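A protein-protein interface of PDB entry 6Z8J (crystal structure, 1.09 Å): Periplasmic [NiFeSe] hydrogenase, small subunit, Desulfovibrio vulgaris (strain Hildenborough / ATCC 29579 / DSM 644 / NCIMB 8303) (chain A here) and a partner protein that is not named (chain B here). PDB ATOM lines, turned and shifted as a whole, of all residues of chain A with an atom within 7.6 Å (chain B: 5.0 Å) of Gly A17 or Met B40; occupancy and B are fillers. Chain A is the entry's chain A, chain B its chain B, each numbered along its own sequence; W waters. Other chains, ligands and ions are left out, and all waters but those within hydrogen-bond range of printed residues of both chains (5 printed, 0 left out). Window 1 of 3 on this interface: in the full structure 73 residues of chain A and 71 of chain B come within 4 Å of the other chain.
The side-chain amide nitrogen of Gln A16 is in hydrogen-bond range of the backbone carbonyl oxygen of Tyr B41 (3.0 Å).
The backbone carbonyl oxygen (O) of Gly B39 is in hydrogen-bond range of the backbone NH (N) of Ile A90, at 2.9 Å.
The side-chain hydroxyl of Thr A19 is in hydrogen-bond range of the side-chain carboxylate of Glu B17, 2.6 Å away.
The backbone NH (N) of Tyr B41 sits at hydrogen-bond distance from the backbone carbonyl oxygen (O) of Tyr A88 (2.9 Å).
O of Gln A14 sits at hydrogen-bond distance from NE2 of His B19, 2.8 Å away.
The backbone NH (N) of Gly B39 sits at hydrogen-bond distance from the backbone carbonyl oxygen (O) of His B19 (3.2 Å).
OE2 of Glu A77 lies close to N of Thr A19.
The backbone carbonyl oxygen (O) of Gly B38 lies within hydrogen-bond range of the backbone NH (N) of Phe B304.
The side-chain carboxylate (OE1) of Glu A77 lies within hydrogen-bond range of the side-chain amide nitrogen (NE2) of Gln A14 (3.1 Å).
NE2 of Gln A16 sits at hydrogen-bond distance from OG1 of Thr A135, 3.0 Å away.
SD of Met B40 sits close to NE of Arg B42, 3.7 Å away.
O of Gly A15 touches CE1 of His B19, at 2.9 Å.
Met B40 touches Gln A16 (SD to CA, 3.8 Å).
CB of Gln A16 touches CG of Arg B42, 3.8 Å away.
OE2 of Glu B17 touches O of Cys A18, 3.6 Å away.
Lys A87 touches Phe B304.
Tyr A88 touches Phe B304.
CE1 of His B19 touches SG of Cys A89, 3.8 Å away.
CA of Cys A89 touches O of Gly B39, 3.4 Å away.
CG of Pro A128 touches CD of Arg B42 (3.98 Å).
Thr A135 touches Tyr B41 (CG2 to CD2, 3.7 Å).
Printed residues of chain B within 4 Å of Gly A15: His B19 (2.9 Å) and Met B40 (3.9 Å).
Gly A17 touches just these residues of chain B: Met B40 and Arg B42.
Gly A20 touches none of the printed residues of chain B.
Of the printed residues of chain B, Cys A89 touches His B19 (3.8 Å), Gly B39 (3.4 Å) and Met B40 (3.6 Å).
Of the printed residues of chain B, Ile A90 touches His B19 and Gly B39.
Of the printed residues of chain B, Ile A91 touches His B19.
Of the printed residues of chain B, Pro A128 touches Arg B42.
Gly B38 touches none of the printed residues of chain A.
Printed residues of chain A within 4 Å of Met B40: Gly A15 (3.9 Å), Gln A16 (3.8 Å), Gly A17 (3.4 Å), Tyr A88 (3.2 Å) and Cys A89 (3.6 Å).
The nearest residue of chain A that does not touch Met B40 is Ile A90 (4.8 Å).
Of the 9 printed residues of chain B, 7 touch a printed residue of chain A.
Hydrophobic or aromatic side chains of chain B that line the printed part of chain A: His B19, Met B40, Tyr B41 and Phe B304.
Printed residues of chain A that touch a printed residue of chain B: Gln A14, Gly A15, Gln A16, Gly A17, Cys A18, Thr A19, Lys A87, Tyr A88, Cys A89, Ile A90, Ile A91, Pro A128 and Thr A135.
Among the printed residues, 24 pairs touch across the chains.
Water W5 lies within hydrogen-bond range of OE2 of Glu B17 (2.6 Å) and O of Gly A17 (2.9 Å).
Water W3 lies within hydrogen-bond range of the side-chain amide oxygen (OE1) of Gln A14 (2.6 Å) and a ring nitrogen (NE2) of His B19 (3.1 Å).
Water W2 lies within hydrogen-bond range of OG1 of Thr A135 (2.7 Å), O of Pro A128 (2.7 Å) and O of Arg B42 (2.8 Å).
Water W1 lies within hydrogen-bond range of NH1 of Arg B42 (2.9 Å) and O of Gln A16 (3.0 Å).
Water W4 lies within hydrogen-bond range of ND1 of His B19 (3.4 Å) and O of Gly A15 (3.4 Å).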
ATOM      1  N   GLN A  14     -19.616 -24.185 -21.472  1.00  0.00           N
ATOM      2  CA  GLN A  14     -20.456 -23.136 -20.915  1.00  0.00           C
ATOM      3  C   GLN A  14     -19.979 -22.801 -19.506  1.00  0.00           C
ATOM      4  O   GLN A  14     -19.917 -23.678 -18.640  1.00  0.00           O
ATOM      5  CB  GLN A  14     -21.923 -23.574 -20.881  1.00  0.00           C
ATOM      6  CG  GLN A  14     -22.445 -23.858 -22.286  1.00  0.00           C
ATOM      7  CD  GLN A  14     -23.772 -24.583 -22.341  1.00  0.00           C
ATOM      8  OE1 GLN A  14     -24.126 -25.366 -21.442  1.00  0.00           O
ATOM      9  NE2 GLN A  14     -24.528 -24.326 -23.413  1.00  0.00           N
ATOM     10  N   GLY A  15     -19.672 -21.529 -19.281  1.00  0.00           N
ATOM     11  CA  GLY A  15     -19.397 -21.000 -17.962  1.00  0.00           C
ATOM     12  C   GLY A  15     -20.647 -20.373 -17.388  1.00  0.00           C
ATOM     13  O   GLY A  15     -21.678 -21.039 -17.249  1.00  0.00           O
ATOM     14  N   GLN A  16     -20.582 -19.088 -17.054  1.00  0.00           N
ATOM     15  CA  GLN A  16     -21.745 -18.363 -16.543  1.00  0.00           C
ATOM     16  C   GLN A  16     -22.517 -17.821 -17.737  1.00  0.00           C
ATOM     17  O   GLN A  16     -22.522 -16.632 -18.016  1.00  0.00           O
ATOM     18  CB  GLN A  16     -21.315 -17.227 -15.629  1.00  0.00           C
ATOM     19  CG  GLN A  16     -20.681 -17.668 -14.337  1.00  0.00           C
ATOM     20  CD  GLN A  16     -20.095 -16.506 -13.575  1.00  0.00           C
ATOM     21  OE1 GLN A  16     -19.190 -15.824 -14.075  1.00  0.00           O
ATOM     22  NE2 GLN A  16     -20.637 -16.230 -12.406  1.00  0.00           N
ATOM     23  N   GLY A  17     -23.166 -18.740 -18.447  1.00  0.00           N
ATOM     24  CA  GLY A  17     -23.975 -18.408 -19.593  1.00  0.00           C
ATOM     25  C   GLY A  17     -25.446 -18.679 -19.315  1.00  0.00           C
ATOM     26  O   GLY A  17     -25.820 -19.259 -18.299  1.00  0.00           O
ATOM     27  N   CYS A  18     -26.285 -18.235 -20.253  1.00  0.00           N
ATOM     28  CA  CYS A  18     -27.712 -18.504 -20.207  1.00  0.00           C
ATOM     29  C   CYS A  18     -28.150 -19.472 -21.284  1.00  0.00           C
ATOM     30  O   CYS A  18     -29.359 -19.705 -21.439  1.00  0.00           O
ATOM     31  CB  CYS A  18     -28.543 -17.217 -20.274  1.00  0.00           C
ATOM     32  SG  CYS A  18     -28.774 -16.500 -21.935  1.00  0.00           S
ATOM     33  N   THR A  19     -27.204 -20.017 -22.052  1.00  0.00           N
ATOM     34  CA  THR A  19     -27.464 -20.904 -23.175  1.00  0.00           C
ATOM     35  C   THR A  19     -28.071 -20.156 -24.368  1.00  0.00           C
ATOM     36  O   THR A  19     -28.359 -20.772 -25.417  1.00  0.00           O
ATOM     37  CB  THR A  19     -28.245 -22.139 -22.712  1.00  0.00           C
ATOM     38  OG1 THR A  19     -27.542 -22.691 -21.588  1.00  0.00           O
ATOM     39  CG2 THR A  19     -28.341 -23.213 -23.773  1.00  0.00           C
ATOM     40  N   GLY A  20     -28.204 -18.837 -24.277  1.00  0.00           N
ATOM     41  CA  GLY A  20     -28.705 -18.057 -25.393  1.00  0.00           C
ATOM     42  C   GLY A  20     -27.809 -18.105 -26.605  1.00  0.00           C
ATOM     43  O   GLY A  20     -28.287 -17.967 -27.735  1.00  0.00           O
ATOM     44  N   CYS A  21     -26.516 -18.288 -26.390  1.00  0.00           N
ATOM     45  CA  CYS A  21     -25.588 -18.328 -27.505  1.00  0.00           C
ATOM     46  C   CYS A  21     -25.660 -19.670 -28.252  1.00  0.00           C
ATOM     47  O   CYS A  21     -25.409 -19.711 -29.462  1.00  0.00           O
ATOM     48  CB  CYS A  21     -24.186 -17.924 -27.006  1.00  0.00           C
ATOM     49  SG  CYS A  21     -23.987 -16.170 -26.395  1.00  0.00           S
ATOM     50  N   GLU A  77     -18.896 -20.099 -23.946  1.00  0.00           N
ATOM     51  CA  GLU A  77     -20.134 -19.343 -23.758  1.00  0.00           C
ATOM     52  C   GLU A  77     -20.234 -19.036 -22.268  1.00  0.00           C
ATOM     53  O   GLU A  77     -20.074 -19.939 -21.455  1.00  0.00           O
ATOM     54  CB  GLU A  77     -21.340 -20.199 -24.235  1.00  0.00           C
ATOM     55  CG  GLU A  77     -22.790 -19.704 -23.867  1.00  0.00           C
ATOM     56  CD  GLU A  77     -23.983 -20.525 -24.486  1.00  0.00           C
ATOM     57  OE1 GLU A  77     -23.922 -21.704 -24.888  1.00  0.00           O
ATOM     58  OE2 GLU A  77     -25.081 -19.941 -24.559  1.00  0.00           O
ATOM     59  N   GLY A  78     -20.459 -17.776 -21.914  1.00  0.00           N
ATOM     60  CA  GLY A  78     -20.504 -17.383 -20.523  1.00  0.00           C
ATOM     61  C   GLY A  78     -19.171 -16.846 -20.014  1.00  0.00           C
ATOM     62  O   GLY A  78     -18.108 -17.091 -20.573  1.00  0.00           O
ATOM     63  N   SER A  79     -19.243 -16.111 -18.909  1.00  0.00           N
ATOM     64  CA  SER A  79     -18.043 -15.623 -18.255  1.00  0.00           C
ATOM     65  C   SER A  79     -17.447 -16.696 -17.343  1.00  0.00           C
ATOM     66  O   SER A  79     -18.059 -17.730 -17.067  1.00  0.00           O
ATOM     67  CB  SER A  79     -18.347 -14.344 -17.481  1.00  0.00           C
ATOM     68  OG  SER A  79     -19.420 -14.553 -16.572  1.00  0.00           O
ATOM     69  N   VAL A  80     -16.243 -16.420 -16.857  1.00  0.00           N
ATOM     70  CA  VAL A  80     -15.479 -17.338 -16.019  1.00  0.00           C
ATOM     71  C   VAL A  80     -15.377 -16.709 -14.634  1.00  0.00           C
ATOM     72  O   VAL A  80     -14.660 -15.713 -14.471  1.00  0.00           O
ATOM     73  CB  VAL A  80     -14.074 -17.566 -16.589  1.00  0.00           C
ATOM     74  CG1 VAL A  80     -13.306 -18.569 -15.718  1.00  0.00           C
ATOM     75  CG2 VAL A  80     -14.152 -17.995 -18.032  1.00  0.00           C
ATOM     76  N   PRO A  81     -16.028 -17.250 -13.614  1.00  0.00           N
ATOM     77  CA  PRO A  81     -15.959 -16.605 -12.298  1.00  0.00           C
ATOM     78  C   PRO A  81     -14.769 -17.107 -11.492  1.00  0.00           C
ATOM     79  O   PRO A  81     -14.609 -18.315 -11.291  1.00  0.00           O
ATOM     80  CB  PRO A  81     -17.291 -16.992 -11.647  1.00  0.00           C
ATOM     81  CG  PRO A  81     -17.637 -18.333 -12.244  1.00  0.00           C
ATOM     82  CD  PRO A  81     -17.027 -18.335 -13.653  1.00  0.00           C
ATOM     83  N   LYS A  87     -15.648 -21.701  -7.403  1.00  0.00           N
ATOM     84  CA  LYS A  87     -16.808 -22.495  -6.992  1.00  0.00           C
ATOM     85  C   LYS A  87     -18.135 -21.977  -7.529  1.00  0.00           C
ATOM     86  O   LYS A  87     -19.127 -22.700  -7.448  1.00  0.00           O
ATOM     87  CB  LYS A  87     -16.883 -22.531  -5.465  1.00  0.00           C
ATOM     88  CG  LYS A  87     -15.959 -23.531  -4.817  1.00  0.00           C
ATOM     89  CD  LYS A  87     -16.219 -23.533  -3.302  1.00  0.00           C
ATOM     90  CE  LYS A  87     -15.308 -24.476  -2.547  1.00  0.00           C
ATOM     91  NZ  LYS A  87     -15.764 -24.638  -1.137  1.00  0.00           N
ATOM     92  N   TYR A  88     -18.191 -20.760  -8.057  1.00  0.00           N
ATOM     93  CA  TYR A  88     -19.429 -20.261  -8.641  1.00  0.00           C
ATOM     94  C   TYR A  88     -19.733 -20.847 -10.019  1.00  0.00           C
ATOM     95  O   TYR A  88     -20.786 -20.546 -10.578  1.00  0.00           O
ATOM     96  CB  TYR A  88     -19.416 -18.734  -8.679  1.00  0.00           C
ATOM     97  CG  TYR A  88     -19.516 -18.075  -7.312  1.00  0.00           C
ATOM     98  CD1 TYR A  88     -20.635 -18.276  -6.511  1.00  0.00           C
ATOM     99  CD2 TYR A  88     -18.511 -17.239  -6.831  1.00  0.00           C
ATOM    100  CE1 TYR A  88     -20.757 -17.668  -5.286  1.00  0.00           C
ATOM    101  CE2 TYR A  88     -18.624 -16.618  -5.590  1.00  0.00           C
ATOM    102  CZ  TYR A  88     -19.751 -16.839  -4.831  1.00  0.00           C
ATOM    103  OH  TYR A  88     -19.877 -16.220  -3.625  1.00  0.00           O
ATOM    104  N   CYS A  89     -18.852 -21.669 -10.589  1.00  0.00           N
ATOM    105  CA  CYS A  89     -19.212 -22.390 -11.812  1.00  0.00           C
ATOM    106  C   CYS A  89     -18.488 -23.734 -11.842  1.00  0.00           C
ATOM    107  O   CYS A  89     -17.337 -23.812 -12.276  1.00  0.00           O
ATOM    108  CB  CYS A  89     -18.905 -21.572 -13.050  1.00  0.00           C
ATOM    109  SG  CYS A  89     -19.559 -22.301 -14.544  1.00  0.00           S
ATOM    110  N   ILE A  90     -19.197 -24.788 -11.452  1.00  0.00           N
ATOM    111  CA  ILE A  90     -18.716 -26.157 -11.568  1.00  0.00           C
ATOM    112  C   ILE A  90     -19.377 -26.757 -12.801  1.00  0.00           C
ATOM    113  O   ILE A  90     -20.607 -26.777 -12.909  1.00  0.00           O
ATOM    114  CB  ILE A  90     -19.046 -26.976 -10.310  1.00  0.00           C
ATOM    115  CG1 ILE A  90     -18.364 -26.371  -9.072  1.00  0.00           C
ATOM    116  CG2 ILE A  90     -18.668 -28.438 -10.514  1.00  0.00           C
ATOM    117  CD1 ILE A  90     -16.880 -26.169  -9.173  1.00  0.00           C
ATOM    118  N   ILE A  91     -18.557 -27.227 -13.743  1.00  0.00           N
ATOM    119  CA  ILE A  91     -19.037 -27.693 -15.044  1.00  0.00           C
ATOM    120  C   ILE A  91     -19.013 -29.207 -15.199  1.00  0.00           C
ATOM    121  O   ILE A  91     -19.530 -29.719 -16.206  1.00  0.00           O
ATOM    122  CB  ILE A  91     -18.273 -27.024 -16.207  1.00  0.00           C
ATOM    123  CG1 ILE A  91     -16.856 -27.577 -16.378  1.00  0.00           C
ATOM    124  CG2 ILE A  91     -18.231 -25.527 -16.009  1.00  0.00           C
ATOM    125  CD1 ILE A  91     -16.232 -27.170 -17.707  1.00  0.00           C
ATOM    126  N   MET A 101     -15.030 -23.989 -14.029  1.00  0.00           N
ATOM    127  CA  MET A 101     -14.745 -23.348 -15.305  1.00  0.00           C
ATOM    128  C   MET A 101     -13.310 -22.843 -15.348  1.00  0.00           C
ATOM    129  O   MET A 101     -12.636 -22.945 -16.383  1.00  0.00           O
ATOM    130  CB  MET A 101     -15.719 -22.212 -15.577  1.00  0.00           C
ATOM    131  CG  MET A 101     -15.544 -21.657 -16.988  1.00  0.00           C
ATOM    132  SD  MET A 101     -15.974 -22.844 -18.297  1.00  0.00           S
ATOM    133  CE  MET A 101     -16.149 -21.712 -19.659  1.00  0.00           C
ATOM    134  N   CYS A 121     -20.930 -12.101 -22.578  1.00  0.00           N
ATOM    135  CA  CYS A 121     -20.399 -12.566 -21.296  1.00  0.00           C
ATOM    136  C   CYS A 121     -18.978 -13.094 -21.456  1.00  0.00           C
ATOM    137  O   CYS A 121     -18.065 -12.700 -20.720  1.00  0.00           O
ATOM    138  CB  CYS A 121     -21.263 -13.678 -20.707  1.00  0.00           C
ATOM    139  SG  CYS A 121     -22.982 -13.252 -20.343  1.00  0.00           S
ATOM    140  N   ALA A 122     -18.783 -14.021 -22.392  1.00  0.00           N
ATOM    141  CA  ALA A 122     -17.462 -14.581 -22.611  1.00  0.00           C
ATOM    142  C   ALA A 122     -16.502 -13.538 -23.162  1.00  0.00           C
ATOM    143  O   ALA A 122     -15.323 -13.523 -22.807  1.00  0.00           O
ATOM    144  CB  ALA A 122     -17.586 -15.756 -23.573  1.00  0.00           C
ATOM    145  N   PRO A 128     -23.041 -10.998 -16.011  1.00  0.00           N
ATOM    146  CA  PRO A 128     -22.497 -11.574 -14.768  1.00  0.00           C
ATOM    147  C   PRO A 128     -21.402 -10.743 -14.120  1.00  0.00           C
ATOM    148  O   PRO A 128     -21.155 -10.913 -12.923  1.00  0.00           O
ATOM    149  CB  PRO A 128     -21.996 -12.958 -15.192  1.00  0.00           C
ATOM    150  CG  PRO A 128     -22.876 -13.310 -16.368  1.00  0.00           C
ATOM    151  CD  PRO A 128     -23.060 -11.990 -17.101  1.00  0.00           C
ATOM    152  N   THR A 135     -19.188 -12.571  -8.146  1.00  0.00           N
ATOM    153  CA  THR A 135     -18.565 -13.855  -8.434  1.00  0.00           C
ATOM    154  C   THR A 135     -17.180 -13.729  -9.086  1.00  0.00           C
ATOM    155  O   THR A 135     -16.562 -14.753  -9.373  1.00  0.00           O
ATOM    156  CB  THR A 135     -19.464 -14.720  -9.332  1.00  0.00           C
ATOM    157  OG1 THR A 135     -19.597 -14.088 -10.610  1.00  0.00           O
ATOM    158  CG2 THR A 135     -20.822 -14.961  -8.693  1.00  0.00           C
ATOM    159  N   GLU B  17     -30.690 -27.685 -20.003  1.00  0.00           N
ATOM    160  CA  GLU B  17     -29.998 -26.406 -19.968  1.00  0.00           C
ATOM    161  C   GLU B  17     -29.292 -26.245 -18.631  1.00  0.00           C
ATOM    162  O   GLU B  17     -29.848 -26.549 -17.570  1.00  0.00           O
ATOM    163  CB  GLU B  17     -30.960 -25.245 -20.186  1.00  0.00           C
ATOM    164  CG  GLU B  17     -30.321 -23.870 -20.332  1.00  0.00           C
ATOM    165  CD  GLU B  17     -29.662 -23.292 -19.070  1.00  0.00           C
ATOM    166  OE1 GLU B  17     -30.138 -23.543 -17.941  1.00  0.00           O
ATOM    167  OE2 GLU B  17     -28.680 -22.519 -19.236  1.00  0.00           O
ATOM    168  N   HIS B  19     -26.128 -26.068 -15.627  1.00  0.00           N
ATOM    169  CA  HIS B  19     -25.138 -26.862 -14.912  1.00  0.00           C
ATOM    170  C   HIS B  19     -25.793 -27.637 -13.777  1.00  0.00           C
ATOM    171  O   HIS B  19     -26.175 -27.049 -12.762  1.00  0.00           O
ATOM    172  CB  HIS B  19     -24.031 -25.956 -14.371  1.00  0.00           C
ATOM    173  CG  HIS B  19     -23.162 -25.370 -15.429  1.00  0.00           C
ATOM    174  ND1 HIS B  19     -23.133 -24.033 -15.766  1.00  0.00           N
ATOM    175  CD2 HIS B  19     -22.295 -25.985 -16.259  1.00  0.00           C
ATOM    176  CE1 HIS B  19     -22.255 -23.854 -16.746  1.00  0.00           C
ATOM    177  NE2 HIS B  19     -21.741 -25.026 -17.068  1.00  0.00           N
ATOM    178  N   GLY B  38     -27.203 -27.668  -8.344  1.00  0.00           N
ATOM    179  CA  GLY B  38     -27.022 -26.648  -9.368  1.00  0.00           C
ATOM    180  C   GLY B  38     -25.703 -25.949  -9.111  1.00  0.00           C
ATOM    181  O   GLY B  38     -25.540 -25.296  -8.082  1.00  0.00           O
ATOM    182  N   GLY B  39     -24.741 -26.111 -10.012  1.00  0.00           N
ATOM    183  CA  GLY B  39     -23.374 -25.736  -9.741  1.00  0.00           C
ATOM    184  C   GLY B  39     -22.902 -24.405 -10.274  1.00  0.00           C
ATOM    185  O   GLY B  39     -21.701 -24.117 -10.164  1.00  0.00           O
ATOM    186  N   MET B  40     -23.784 -23.575 -10.831  1.00  0.00           N
ATOM    187  CA  MET B  40     -23.366 -22.282 -11.364  1.00  0.00           C
ATOM    188  C   MET B  40     -24.288 -21.180 -10.870  1.00  0.00           C
ATOM    189  O   MET B  40     -25.508 -21.317 -10.928  1.00  0.00           O
ATOM    190  CB  MET B  40     -23.289 -22.297 -12.893  1.00  0.00           C
ATOM    191  CG  MET B  40     -22.758 -20.998 -13.501  1.00  0.00           C
ATOM    192  SD  MET B  40     -23.977 -19.681 -13.747  1.00  0.00           S
ATOM    193  CE  MET B  40     -24.859 -20.279 -15.192  1.00  0.00           C
ATOM    194  N   TYR B  41     -23.687 -20.088 -10.396  1.00  0.00           N
ATOM    195  CA  TYR B  41     -24.413 -18.953  -9.861  1.00  0.00           C
ATOM    196  C   TYR B  41     -23.946 -17.656 -10.505  1.00  0.00           C
ATOM    197  O   TYR B  41     -22.754 -17.457 -10.735  1.00  0.00           O
ATOM    198  CB  TYR B  41     -24.176 -18.886  -8.349  1.00  0.00           C
ATOM    199  CG  TYR B  41     -24.729 -17.668  -7.638  1.00  0.00           C
ATOM    200  CD1 TYR B  41     -26.055 -17.620  -7.222  1.00  0.00           C
ATOM    201  CD2 TYR B  41     -23.921 -16.569  -7.368  1.00  0.00           C
ATOM    202  CE1 TYR B  41     -26.553 -16.508  -6.542  1.00  0.00           C
ATOM    203  CE2 TYR B  41     -24.407 -15.459  -6.705  1.00  0.00           C
ATOM    204  CZ  TYR B  41     -25.727 -15.424  -6.288  1.00  0.00           C
ATOM    205  OH  TYR B  41     -26.212 -14.331  -5.608  1.00  0.00           O
ATOM    206  N   ARG B  42     -24.909 -16.768 -10.767  1.00  0.00           N
ATOM    207  CA  ARG B  42     -24.644 -15.426 -11.259  1.00  0.00           C
ATOM    208  C   ARG B  42     -25.137 -14.323 -10.337  1.00  0.00           C
ATOM    209  O   ARG B  42     -24.467 -13.300 -10.212  1.00  0.00           O
ATOM    210  CB  ARG B  42     -25.242 -15.260 -12.650  1.00  0.00           C
ATOM    211  CG  ARG B  42     -24.425 -16.031 -13.707  1.00  0.00           C
ATOM    212  CD  ARG B  42     -25.157 -16.287 -15.037  1.00  0.00           C
ATOM    213  NE  ARG B  42     -26.380 -17.033 -14.843  1.00  0.00           N
ATOM    214  CZ  ARG B  42     -27.406 -17.054 -15.683  1.00  0.00           C
ATOM    215  NH1 ARG B  42     -27.350 -16.390 -16.837  1.00  0.00           N
ATOM    216  NH2 ARG B  42     -28.499 -17.717 -15.341  1.00  0.00           N
ATOM    217  N   PHE B 304     -26.634 -24.276  -5.531  1.00  0.00           N
ATOM    218  CA  PHE B 304     -26.980 -22.861  -5.606  1.00  0.00           C
ATOM    219  C   PHE B 304     -28.469 -22.614  -5.840  1.00  0.00           C
ATOM    220  O   PHE B 304     -28.899 -21.453  -5.924  1.00  0.00           O
ATOM    221  CB  PHE B 304     -26.165 -22.149  -6.694  1.00  0.00           C
ATOM    222  CG  PHE B 304     -24.718 -21.945  -6.348  1.00  0.00           C
ATOM    223  CD1 PHE B 304     -24.352 -21.097  -5.334  1.00  0.00           C
ATOM    224  CD2 PHE B 304     -23.727 -22.578  -7.079  1.00  0.00           C
ATOM    225  CE1 PHE B 304     -23.027 -20.895  -5.021  1.00  0.00           C
ATOM    226  CE2 PHE B 304     -22.399 -22.390  -6.792  1.00  0.00           C
ATOM    227  CZ  PHE B 304     -22.040 -21.548  -5.747  1.00  0.00           C
ATOM    228  N   VAL B 483     -31.186 -21.193 -10.608  1.00  0.00           N
ATOM    229  CA  VAL B 483     -30.250 -20.478  -9.745  1.00  0.00           C
ATOM    230  C   VAL B 483     -30.311 -18.971  -9.952  1.00  0.00           C
ATOM    231  O   VAL B 483     -30.264 -18.205  -8.984  1.00  0.00           O
ATOM    232  CB  VAL B 483     -28.808 -20.972  -9.975  1.00  0.00           C
ATOM    233  CG1 VAL B 483     -27.869 -20.171  -9.097  1.00  0.00           C
ATOM    234  CG2 VAL B 483     -28.688 -22.458  -9.708  1.00  0.00           C
HETATM  235  O   HOH W   1     -25.123 -15.238 -18.237  1.00  0.00           O
HETATM  236  O   HOH W   2     -21.933 -12.943 -11.296  1.00  0.00           O
HETATM  237  O   HOH W   3     -24.298 -25.385 -18.839  1.00  0.00           O
HETATM  238  O   HOH W   4     -24.430 -22.542 -18.472  1.00  0.00           O
HETATM  239  O   HOH W   5     -27.047 -21.702 -17.397  1.00  0.00           O
